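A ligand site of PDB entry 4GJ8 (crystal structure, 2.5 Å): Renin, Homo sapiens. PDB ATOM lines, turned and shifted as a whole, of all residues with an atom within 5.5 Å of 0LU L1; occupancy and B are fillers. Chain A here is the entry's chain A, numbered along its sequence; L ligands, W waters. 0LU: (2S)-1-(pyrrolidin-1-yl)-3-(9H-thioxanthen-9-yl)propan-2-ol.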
ATOM      1  N   THR A  18      -9.312  11.323  -6.372  1.00  0.00           N
ATOM      2  CA  THR A  18     -10.108  10.247  -5.795  1.00  0.00           C
ATOM      3  C   THR A  18     -11.396  10.734  -5.110  1.00  0.00           C
ATOM      4  O   THR A  18     -12.345   9.964  -4.971  1.00  0.00           O
ATOM      5  CB  THR A  18      -9.256   9.345  -4.863  1.00  0.00           C
ATOM      6  OG1 THR A  18      -8.679  10.120  -3.826  1.00  0.00           O
ATOM      7  CG2 THR A  18      -8.177   8.630  -5.586  1.00  0.00           C
ATOM      8  N   GLN A  19     -11.409  11.988  -4.639  1.00  0.00           N
ATOM      9  CA  GLN A  19     -12.574  12.529  -3.936  1.00  0.00           C
ATOM     10  C   GLN A  19     -12.901  13.904  -4.473  1.00  0.00           C
ATOM     11  O   GLN A  19     -12.058  14.798  -4.478  1.00  0.00           O
ATOM     12  CB  GLN A  19     -12.299  12.598  -2.440  1.00  0.00           C
ATOM     13  CG  GLN A  19     -12.125  11.249  -1.740  1.00  0.00           C
ATOM     14  CD  GLN A  19     -11.721  11.406  -0.288  1.00  0.00           C
ATOM     15  OE1 GLN A  19     -12.277  12.225   0.449  1.00  0.00           O
ATOM     16  NE2 GLN A  19     -10.765  10.612   0.162  1.00  0.00           N
ATOM     17  N   VAL A  36     -19.949  14.524  -1.140  1.00  0.00           N
ATOM     18  CA  VAL A  36     -19.727  13.857  -2.424  1.00  0.00           C
ATOM     19  C   VAL A  36     -21.148  13.699  -3.050  1.00  0.00           C
ATOM     20  O   VAL A  36     -22.074  13.289  -2.355  1.00  0.00           O
ATOM     21  CB  VAL A  36     -19.003  12.506  -2.218  1.00  0.00           C
ATOM     22  CG1 VAL A  36     -19.352  11.515  -3.293  1.00  0.00           C
ATOM     23  CG2 VAL A  36     -17.499  12.702  -2.115  1.00  0.00           C
ATOM     24  N   ASP A  38     -23.171  11.552  -5.303  1.00  0.00           N
ATOM     25  CA  ASP A  38     -23.003  10.164  -5.712  1.00  0.00           C
ATOM     26  C   ASP A  38     -24.190   9.538  -6.443  1.00  0.00           C
ATOM     27  O   ASP A  38     -25.245   9.341  -5.854  1.00  0.00           O
ATOM     28  CB  ASP A  38     -22.544   9.365  -4.466  1.00  0.00           C
ATOM     29  CG  ASP A  38     -22.601   7.852  -4.519  1.00  0.00           C
ATOM     30  OD1 ASP A  38     -22.134   7.282  -5.519  1.00  0.00           O
ATOM     31  OD2 ASP A  38     -22.979   7.238  -3.516  1.00  0.00           O
ATOM     32  N   TYR A  83     -22.050   1.082   2.046  1.00  0.00           N
ATOM     33  CA  TYR A  83     -21.271   1.472   0.856  1.00  0.00           C
ATOM     34  C   TYR A  83     -20.203   0.397   0.633  1.00  0.00           C
ATOM     35  O   TYR A  83     -19.957  -0.404   1.547  1.00  0.00           O
ATOM     36  CB  TYR A  83     -20.618   2.858   0.992  1.00  0.00           C
ATOM     37  CG  TYR A  83     -21.639   3.957   1.149  1.00  0.00           C
ATOM     38  CD1 TYR A  83     -22.293   4.479   0.041  1.00  0.00           C
ATOM     39  CD2 TYR A  83     -21.984   4.444   2.399  1.00  0.00           C
ATOM     40  CE1 TYR A  83     -23.274   5.455   0.172  1.00  0.00           C
ATOM     41  CE2 TYR A  83     -22.955   5.431   2.549  1.00  0.00           C
ATOM     42  CZ  TYR A  83     -23.595   5.928   1.433  1.00  0.00           C
ATOM     43  OH  TYR A  83     -24.574   6.883   1.554  1.00  0.00           O
ATOM     44  N   THR A  85     -16.997   0.665   0.501  1.00  0.00           N
ATOM     45  CA  THR A  85     -15.943   1.094   1.418  1.00  0.00           C
ATOM     46  C   THR A  85     -16.270   0.908   2.893  1.00  0.00           C
ATOM     47  O   THR A  85     -15.417   0.422   3.651  1.00  0.00           O
ATOM     48  CB  THR A  85     -15.671   2.561   1.108  1.00  0.00           C
ATOM     49  OG1 THR A  85     -16.188   2.879  -0.199  1.00  0.00           O
ATOM     50  CG2 THR A  85     -14.215   2.939   1.229  1.00  0.00           C
ATOM     51  N   GLY A  86     -17.462   1.323   3.305  1.00  0.00           N
ATOM     52  CA  GLY A  86     -17.872   1.235   4.700  1.00  0.00           C
ATOM     53  C   GLY A  86     -19.350   1.464   4.956  1.00  0.00           C
ATOM     54  O   GLY A  86     -20.077   1.855   4.050  1.00  0.00           O
ATOM     55  N   PRO A 118     -13.500   3.392   6.906  1.00  0.00           N
ATOM     56  CA  PRO A 118     -12.613   4.262   6.127  1.00  0.00           C
ATOM     57  C   PRO A 118     -12.813   5.773   6.287  1.00  0.00           C
ATOM     58  O   PRO A 118     -12.088   6.533   5.635  1.00  0.00           O
ATOM     59  CB  PRO A 118     -12.990   3.861   4.701  1.00  0.00           C
ATOM     60  CG  PRO A 118     -14.519   3.658   4.796  1.00  0.00           C
ATOM     61  CD  PRO A 118     -14.750   3.089   6.179  1.00  0.00           C
ATOM     62  N   PHE A 119     -13.785   6.216   7.116  1.00  0.00           N
ATOM     63  CA  PHE A 119     -14.220   7.615   7.241  1.00  0.00           C
ATOM     64  C   PHE A 119     -13.241   8.680   7.722  1.00  0.00           C
ATOM     65  O   PHE A 119     -13.457   9.857   7.479  1.00  0.00           O
ATOM     66  CB  PHE A 119     -15.613   7.718   7.854  1.00  0.00           C
ATOM     67  CG  PHE A 119     -16.643   7.006   7.001  1.00  0.00           C
ATOM     68  CD1 PHE A 119     -17.072   7.549   5.786  1.00  0.00           C
ATOM     69  CD2 PHE A 119     -17.152   5.763   7.384  1.00  0.00           C
ATOM     70  CE1 PHE A 119     -17.984   6.865   4.983  1.00  0.00           C
ATOM     71  CE2 PHE A 119     -18.064   5.079   6.581  1.00  0.00           C
ATOM     72  CZ  PHE A 119     -18.475   5.636   5.390  1.00  0.00           C
ATOM     73  N   LEU A 121     -10.304   8.792   6.412  1.00  0.00           N
ATOM     74  CA  LEU A 121      -9.735   9.052   5.105  1.00  0.00           C
ATOM     75  C   LEU A 121     -10.628   9.911   4.197  1.00  0.00           C
ATOM     76  O   LEU A 121     -10.154  10.410   3.165  1.00  0.00           O
ATOM     77  CB  LEU A 121      -9.371   7.734   4.420  1.00  0.00           C
ATOM     78  CG  LEU A 121      -8.429   6.807   5.217  1.00  0.00           C
ATOM     79  CD1 LEU A 121      -8.342   5.450   4.566  1.00  0.00           C
ATOM     80  CD2 LEU A 121      -7.050   7.418   5.372  1.00  0.00           C
ATOM     81  N   ALA A 122     -11.893  10.147   4.590  1.00  0.00           N
ATOM     82  CA  ALA A 122     -12.824  11.000   3.853  1.00  0.00           C
ATOM     83  C   ALA A 122     -12.478  12.446   4.146  1.00  0.00           C
ATOM     84  O   ALA A 122     -12.254  12.785   5.309  1.00  0.00           O
ATOM     85  CB  ALA A 122     -14.254  10.693   4.261  1.00  0.00           C
ATOM     86  N   PHE A 124     -14.504  14.779   2.817  1.00  0.00           N
ATOM     87  CA  PHE A 124     -15.874  15.255   2.801  1.00  0.00           C
ATOM     88  C   PHE A 124     -16.543  14.836   4.126  1.00  0.00           C
ATOM     89  O   PHE A 124     -16.118  13.856   4.762  1.00  0.00           O
ATOM     90  CB  PHE A 124     -16.635  14.645   1.594  1.00  0.00           C
ATOM     91  CG  PHE A 124     -16.607  13.128   1.518  1.00  0.00           C
ATOM     92  CD1 PHE A 124     -15.596  12.469   0.837  1.00  0.00           C
ATOM     93  CD2 PHE A 124     -17.612  12.371   2.109  1.00  0.00           C
ATOM     94  CE1 PHE A 124     -15.583  11.068   0.744  1.00  0.00           C
ATOM     95  CE2 PHE A 124     -17.577  10.976   2.038  1.00  0.00           C
ATOM     96  CZ  PHE A 124     -16.578  10.339   1.340  1.00  0.00           C
ATOM     97  N   VAL A 127     -22.656  12.481   2.287  1.00  0.00           N
ATOM     98  CA  VAL A 127     -22.977  12.082   0.914  1.00  0.00           C
ATOM     99  C   VAL A 127     -24.368  12.573   0.482  1.00  0.00           C
ATOM    100  O   VAL A 127     -25.303  12.511   1.267  1.00  0.00           O
ATOM    101  CB  VAL A 127     -22.776  10.540   0.705  1.00  0.00           C
ATOM    102  CG1 VAL A 127     -23.255  10.085  -0.664  1.00  0.00           C
ATOM    103  CG2 VAL A 127     -21.319  10.157   0.921  1.00  0.00           C
ATOM    104  N   GLY A 228     -19.573   8.648  -7.336  1.00  0.00           N
ATOM    105  CA  GLY A 228     -18.993   8.445  -6.011  1.00  0.00           C
ATOM    106  C   GLY A 228     -17.818   7.492  -5.979  1.00  0.00           C
ATOM    107  O   GLY A 228     -17.120   7.422  -4.968  1.00  0.00           O
ATOM    108  N   ALA A 229     -17.639   6.713  -7.065  1.00  0.00           N
ATOM    109  CA  ALA A 229     -16.543   5.769  -7.238  1.00  0.00           C
ATOM    110  C   ALA A 229     -15.295   6.528  -7.696  1.00  0.00           C
ATOM    111  O   ALA A 229     -15.371   7.391  -8.574  1.00  0.00           O
ATOM    112  CB  ALA A 229     -16.918   4.725  -8.266  1.00  0.00           C
ATOM    113  N   SER A 230     -14.140   6.232  -7.099  1.00  0.00           N
ATOM    114  CA  SER A 230     -12.917   6.910  -7.467  1.00  0.00           C
ATOM    115  C   SER A 230     -12.336   6.353  -8.749  1.00  0.00           C
ATOM    116  O   SER A 230     -11.671   7.063  -9.501  1.00  0.00           O
ATOM    117  CB  SER A 230     -11.896   6.763  -6.349  1.00  0.00           C
ATOM    118  OG  SER A 230     -12.348   7.390  -5.167  1.00  0.00           O
ATOM    119  N   TYR A 231     -12.576   5.084  -8.991  1.00  0.00           N
ATOM    120  CA  TYR A 231     -11.950   4.382 -10.078  1.00  0.00           C
ATOM    121  C   TYR A 231     -12.907   3.728 -11.053  1.00  0.00           C
ATOM    122  O   TYR A 231     -14.117   3.868 -10.969  1.00  0.00           O
ATOM    123  CB  TYR A 231     -11.084   3.254  -9.462  1.00  0.00           C
ATOM    124  CG  TYR A 231      -9.964   3.713  -8.557  1.00  0.00           C
ATOM    125  CD1 TYR A 231      -9.329   4.945  -8.757  1.00  0.00           C
ATOM    126  CD2 TYR A 231      -9.453   2.873  -7.570  1.00  0.00           C
ATOM    127  CE1 TYR A 231      -8.297   5.367  -7.932  1.00  0.00           C
ATOM    128  CE2 TYR A 231      -8.375   3.268  -6.768  1.00  0.00           C
ATOM    129  CZ  TYR A 231      -7.817   4.528  -6.931  1.00  0.00           C
ATOM    130  OH  TYR A 231      -6.751   4.909  -6.140  1.00  0.00           O
ATOM    131  N   HIS A 301      -9.536  -0.915 -10.155  1.00  0.00           N
ATOM    132  CA  HIS A 301      -9.542  -1.893  -9.070  1.00  0.00           C
ATOM    133  C   HIS A 301     -10.683  -2.870  -9.186  1.00  0.00           C
ATOM    134  O   HIS A 301     -11.434  -2.787 -10.148  1.00  0.00           O
ATOM    135  CB  HIS A 301      -9.464  -1.173  -7.714  1.00  0.00           C
ATOM    136  CG  HIS A 301     -10.723  -0.674  -7.049  1.00  0.00           C
ATOM    137  ND1 HIS A 301     -10.828  -0.763  -5.667  1.00  0.00           N
ATOM    138  CD2 HIS A 301     -11.829  -0.043  -7.522  1.00  0.00           C
ATOM    139  CE1 HIS A 301     -11.982  -0.191  -5.338  1.00  0.00           C
ATOM    140  NE2 HIS A 301     -12.642   0.244  -6.410  1.00  0.00           N
ATOM    141  N   MET A 303     -14.193  -4.447  -7.587  1.00  0.00           N
ATOM    142  CA  MET A 303     -15.278  -4.212  -6.653  1.00  0.00           C
ATOM    143  C   MET A 303     -16.368  -5.190  -7.009  1.00  0.00           C
ATOM    144  O   MET A 303     -16.790  -5.224  -8.173  1.00  0.00           O
ATOM    145  CB  MET A 303     -15.780  -2.761  -6.696  1.00  0.00           C
ATOM    146  CG  MET A 303     -16.585  -2.353  -5.464  1.00  0.00           C
ATOM    147  SD  MET A 303     -15.862  -2.872  -3.835  1.00  0.00           S
ATOM    148  CE  MET A 303     -14.628  -1.599  -3.578  1.00  0.00           C
HETATM  149  C1  0LU L   1     -17.112   7.283  -0.901  1.00  0.00           C
HETATM  150  C2  0LU L   1     -15.568   7.182  -0.991  1.00  0.00           C
HETATM  151  C3  0LU L   1     -17.854   6.729   0.161  1.00  0.00           C
HETATM  152  C4  0LU L   1     -17.834   7.933  -1.931  1.00  0.00           C
HETATM  153  C5  0LU L   1     -14.864   7.240   0.374  1.00  0.00           C
HETATM  154  C6  0LU L   1     -15.208   5.836  -1.669  1.00  0.00           C
HETATM  155  S7  0LU L   1     -17.039   5.894   1.486  1.00  0.00           S
HETATM  156  C8  0LU L   1     -19.263   6.791   0.204  1.00  0.00           C
HETATM  157  C9  0LU L   1     -19.236   7.991  -1.899  1.00  0.00           C
HETATM  158  C10 0LU L   1     -15.455   6.693   1.532  1.00  0.00           C
HETATM  159  C11 0LU L   1     -13.601   7.844   0.457  1.00  0.00           C
HETATM  160  C12 0LU L   1     -13.870   5.898  -2.448  1.00  0.00           C
HETATM  161  C13 0LU L   1     -19.964   7.412  -0.846  1.00  0.00           C
HETATM  162  C14 0LU L   1     -14.793   6.759   2.761  1.00  0.00           C
HETATM  163  C15 0LU L   1     -12.944   7.918   1.689  1.00  0.00           C
HETATM  164  C16 0LU L   1     -12.815   4.998  -1.754  1.00  0.00           C
HETATM  165  O17 0LU L   1     -14.140   5.446  -3.786  1.00  0.00           O
HETATM  166  C18 0LU L   1     -13.532   7.376   2.838  1.00  0.00           C
HETATM  167  N19 0LU L   1     -11.818   4.424  -2.687  1.00  0.00           N
HETATM  168  C20 0LU L   1     -10.421   4.893  -2.619  1.00  0.00           C
HETATM  169  C21 0LU L   1     -11.762   2.964  -2.888  1.00  0.00           C
HETATM  170  C22 0LU L   1      -9.629   3.877  -3.475  1.00  0.00           C
HETATM  171  C23 0LU L   1     -10.713   2.914  -4.019  1.00  0.00           C
HETATM  172  C1  0LU L   2      -8.315   5.058   0.905  1.00  0.00           C
HETATM  173  C2  0LU L   2      -6.969   5.710   0.504  1.00  0.00           C
HETATM  174  C3  0LU L   2      -8.438   3.646   1.090  1.00  0.00           C
HETATM  175  C4  0LU L   2      -9.444   5.863   1.114  1.00  0.00           C
HETATM  176  C5  0LU L   2      -5.800   5.034   1.264  1.00  0.00           C
HETATM  177  C6  0LU L   2      -6.803   5.664  -1.054  1.00  0.00           C
HETATM  178  S7  0LU L   2      -7.050   2.543   0.893  1.00  0.00           S
HETATM  179  C8  0LU L   2      -9.678   3.087   1.465  1.00  0.00           C
HETATM  180  C9  0LU L   2     -10.679   5.296   1.487  1.00  0.00           C
HETATM  181  C10 0LU L   2      -5.750   3.627   1.480  1.00  0.00           C
HETATM  182  C11 0LU L   2      -4.764   5.841   1.795  1.00  0.00           C
HETATM  183  C12 0LU L   2      -5.715   6.590  -1.687  1.00  0.00           C
HETATM  184  C13 0LU L   2     -10.798   3.912   1.664  1.00  0.00           C
HETATM  185  C14 0LU L   2      -4.676   3.052   2.203  1.00  0.00           C
HETATM  186  C15 0LU L   2      -3.686   5.250   2.500  1.00  0.00           C
HETATM  187  C16 0LU L   2      -5.524   6.332  -3.216  1.00  0.00           C
HETATM  188  O17 0LU L   2      -6.028   7.978  -1.461  1.00  0.00           O
HETATM  189  C18 0LU L   2      -3.627   3.863   2.706  1.00  0.00           C
HETATM  190  N19 0LU L   2      -4.239   6.765  -3.861  1.00  0.00           N
HETATM  191  C20 0LU L   2      -4.206   6.690  -5.347  1.00  0.00           C
HETATM  192  C21 0LU L   2      -3.592   8.062  -3.573  1.00  0.00           C
HETATM  193  C22 0LU L   2      -4.118   8.144  -5.869  1.00  0.00           C
HETATM  194  C23 0LU L   2      -4.204   9.021  -4.624  1.00  0.00           C
HETATM  195  O   HOH W   1      -9.868   7.999  -1.609  1.00  0.00           O
HETATM  196  O   HOH W   2     -15.703   3.319  -4.209  1.00  0.00           O
HETATM  197  O   HOH W   3     -13.976   3.173  -6.316  1.00  0.00           O
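OD1 of Asp 38 lies close to N of Gly 228 (3.4 Å). O of Leu 121 is in hydrogen-bond range of NE2 of Gln 19, 3.1 Å away. The side-chain hydroxyl (OG) of Ser 230 lies within hydrogen-bond range of the backbone carbonyl oxygen (O) of Thr 18 (2.6 Å).
The side-chain hydroxyl (OG) of Ser 230 lies within hydrogen-bond range of an oxygen (O17) of 0LU L1, 3.0 Å away. An oxygen (O17) of 0LU L1 is in hydrogen-bond range of the backbone NH (N) of Ser 230, at 3.4 Å. The side-chain hydroxyl of Thr 85 sits close to a sulfur (S7) of 0LU L1, at 3.6 Å.
Gln 19 touches 0LU L1 (NE2 to C15, 3.8 Å). Val 36 touches 0LU L1 (CG1 to C9, 3.8 Å). Tyr 83 touches 0LU L1 (CD1 to C8, 3.8 Å). Pro 118 touches 0LU L1. Phe 119 touches 0LU L1 (CE1 to S7, 3.8 Å). C of Leu 121 touches C15 of 0LU L1, at 3.95 Å. N of Ala 122 touches C18 of 0LU L1, 3.7 Å away. CZ of Phe 124 touches C5 of 0LU L1, at 3.7 Å. Val 127 touches 0LU L1. O of Gly 228 touches C4 of 0LU L1, at 3.2 Å. Tyr 231 touches 0LU L1 (CE2 to C22, 3.6 Å). CE1 of His 301 touches C23 of 0LU L1, 3.6 Å away.
Water W1 bridges the side-chain amide nitrogen (NE2) of Gln 19 and the side-chain hydroxyl (OG1) of Thr 18. Water W3 lies within hydrogen-bond range of N of Ser 230, NE2 of His 301 and O17 of 0LU L1.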
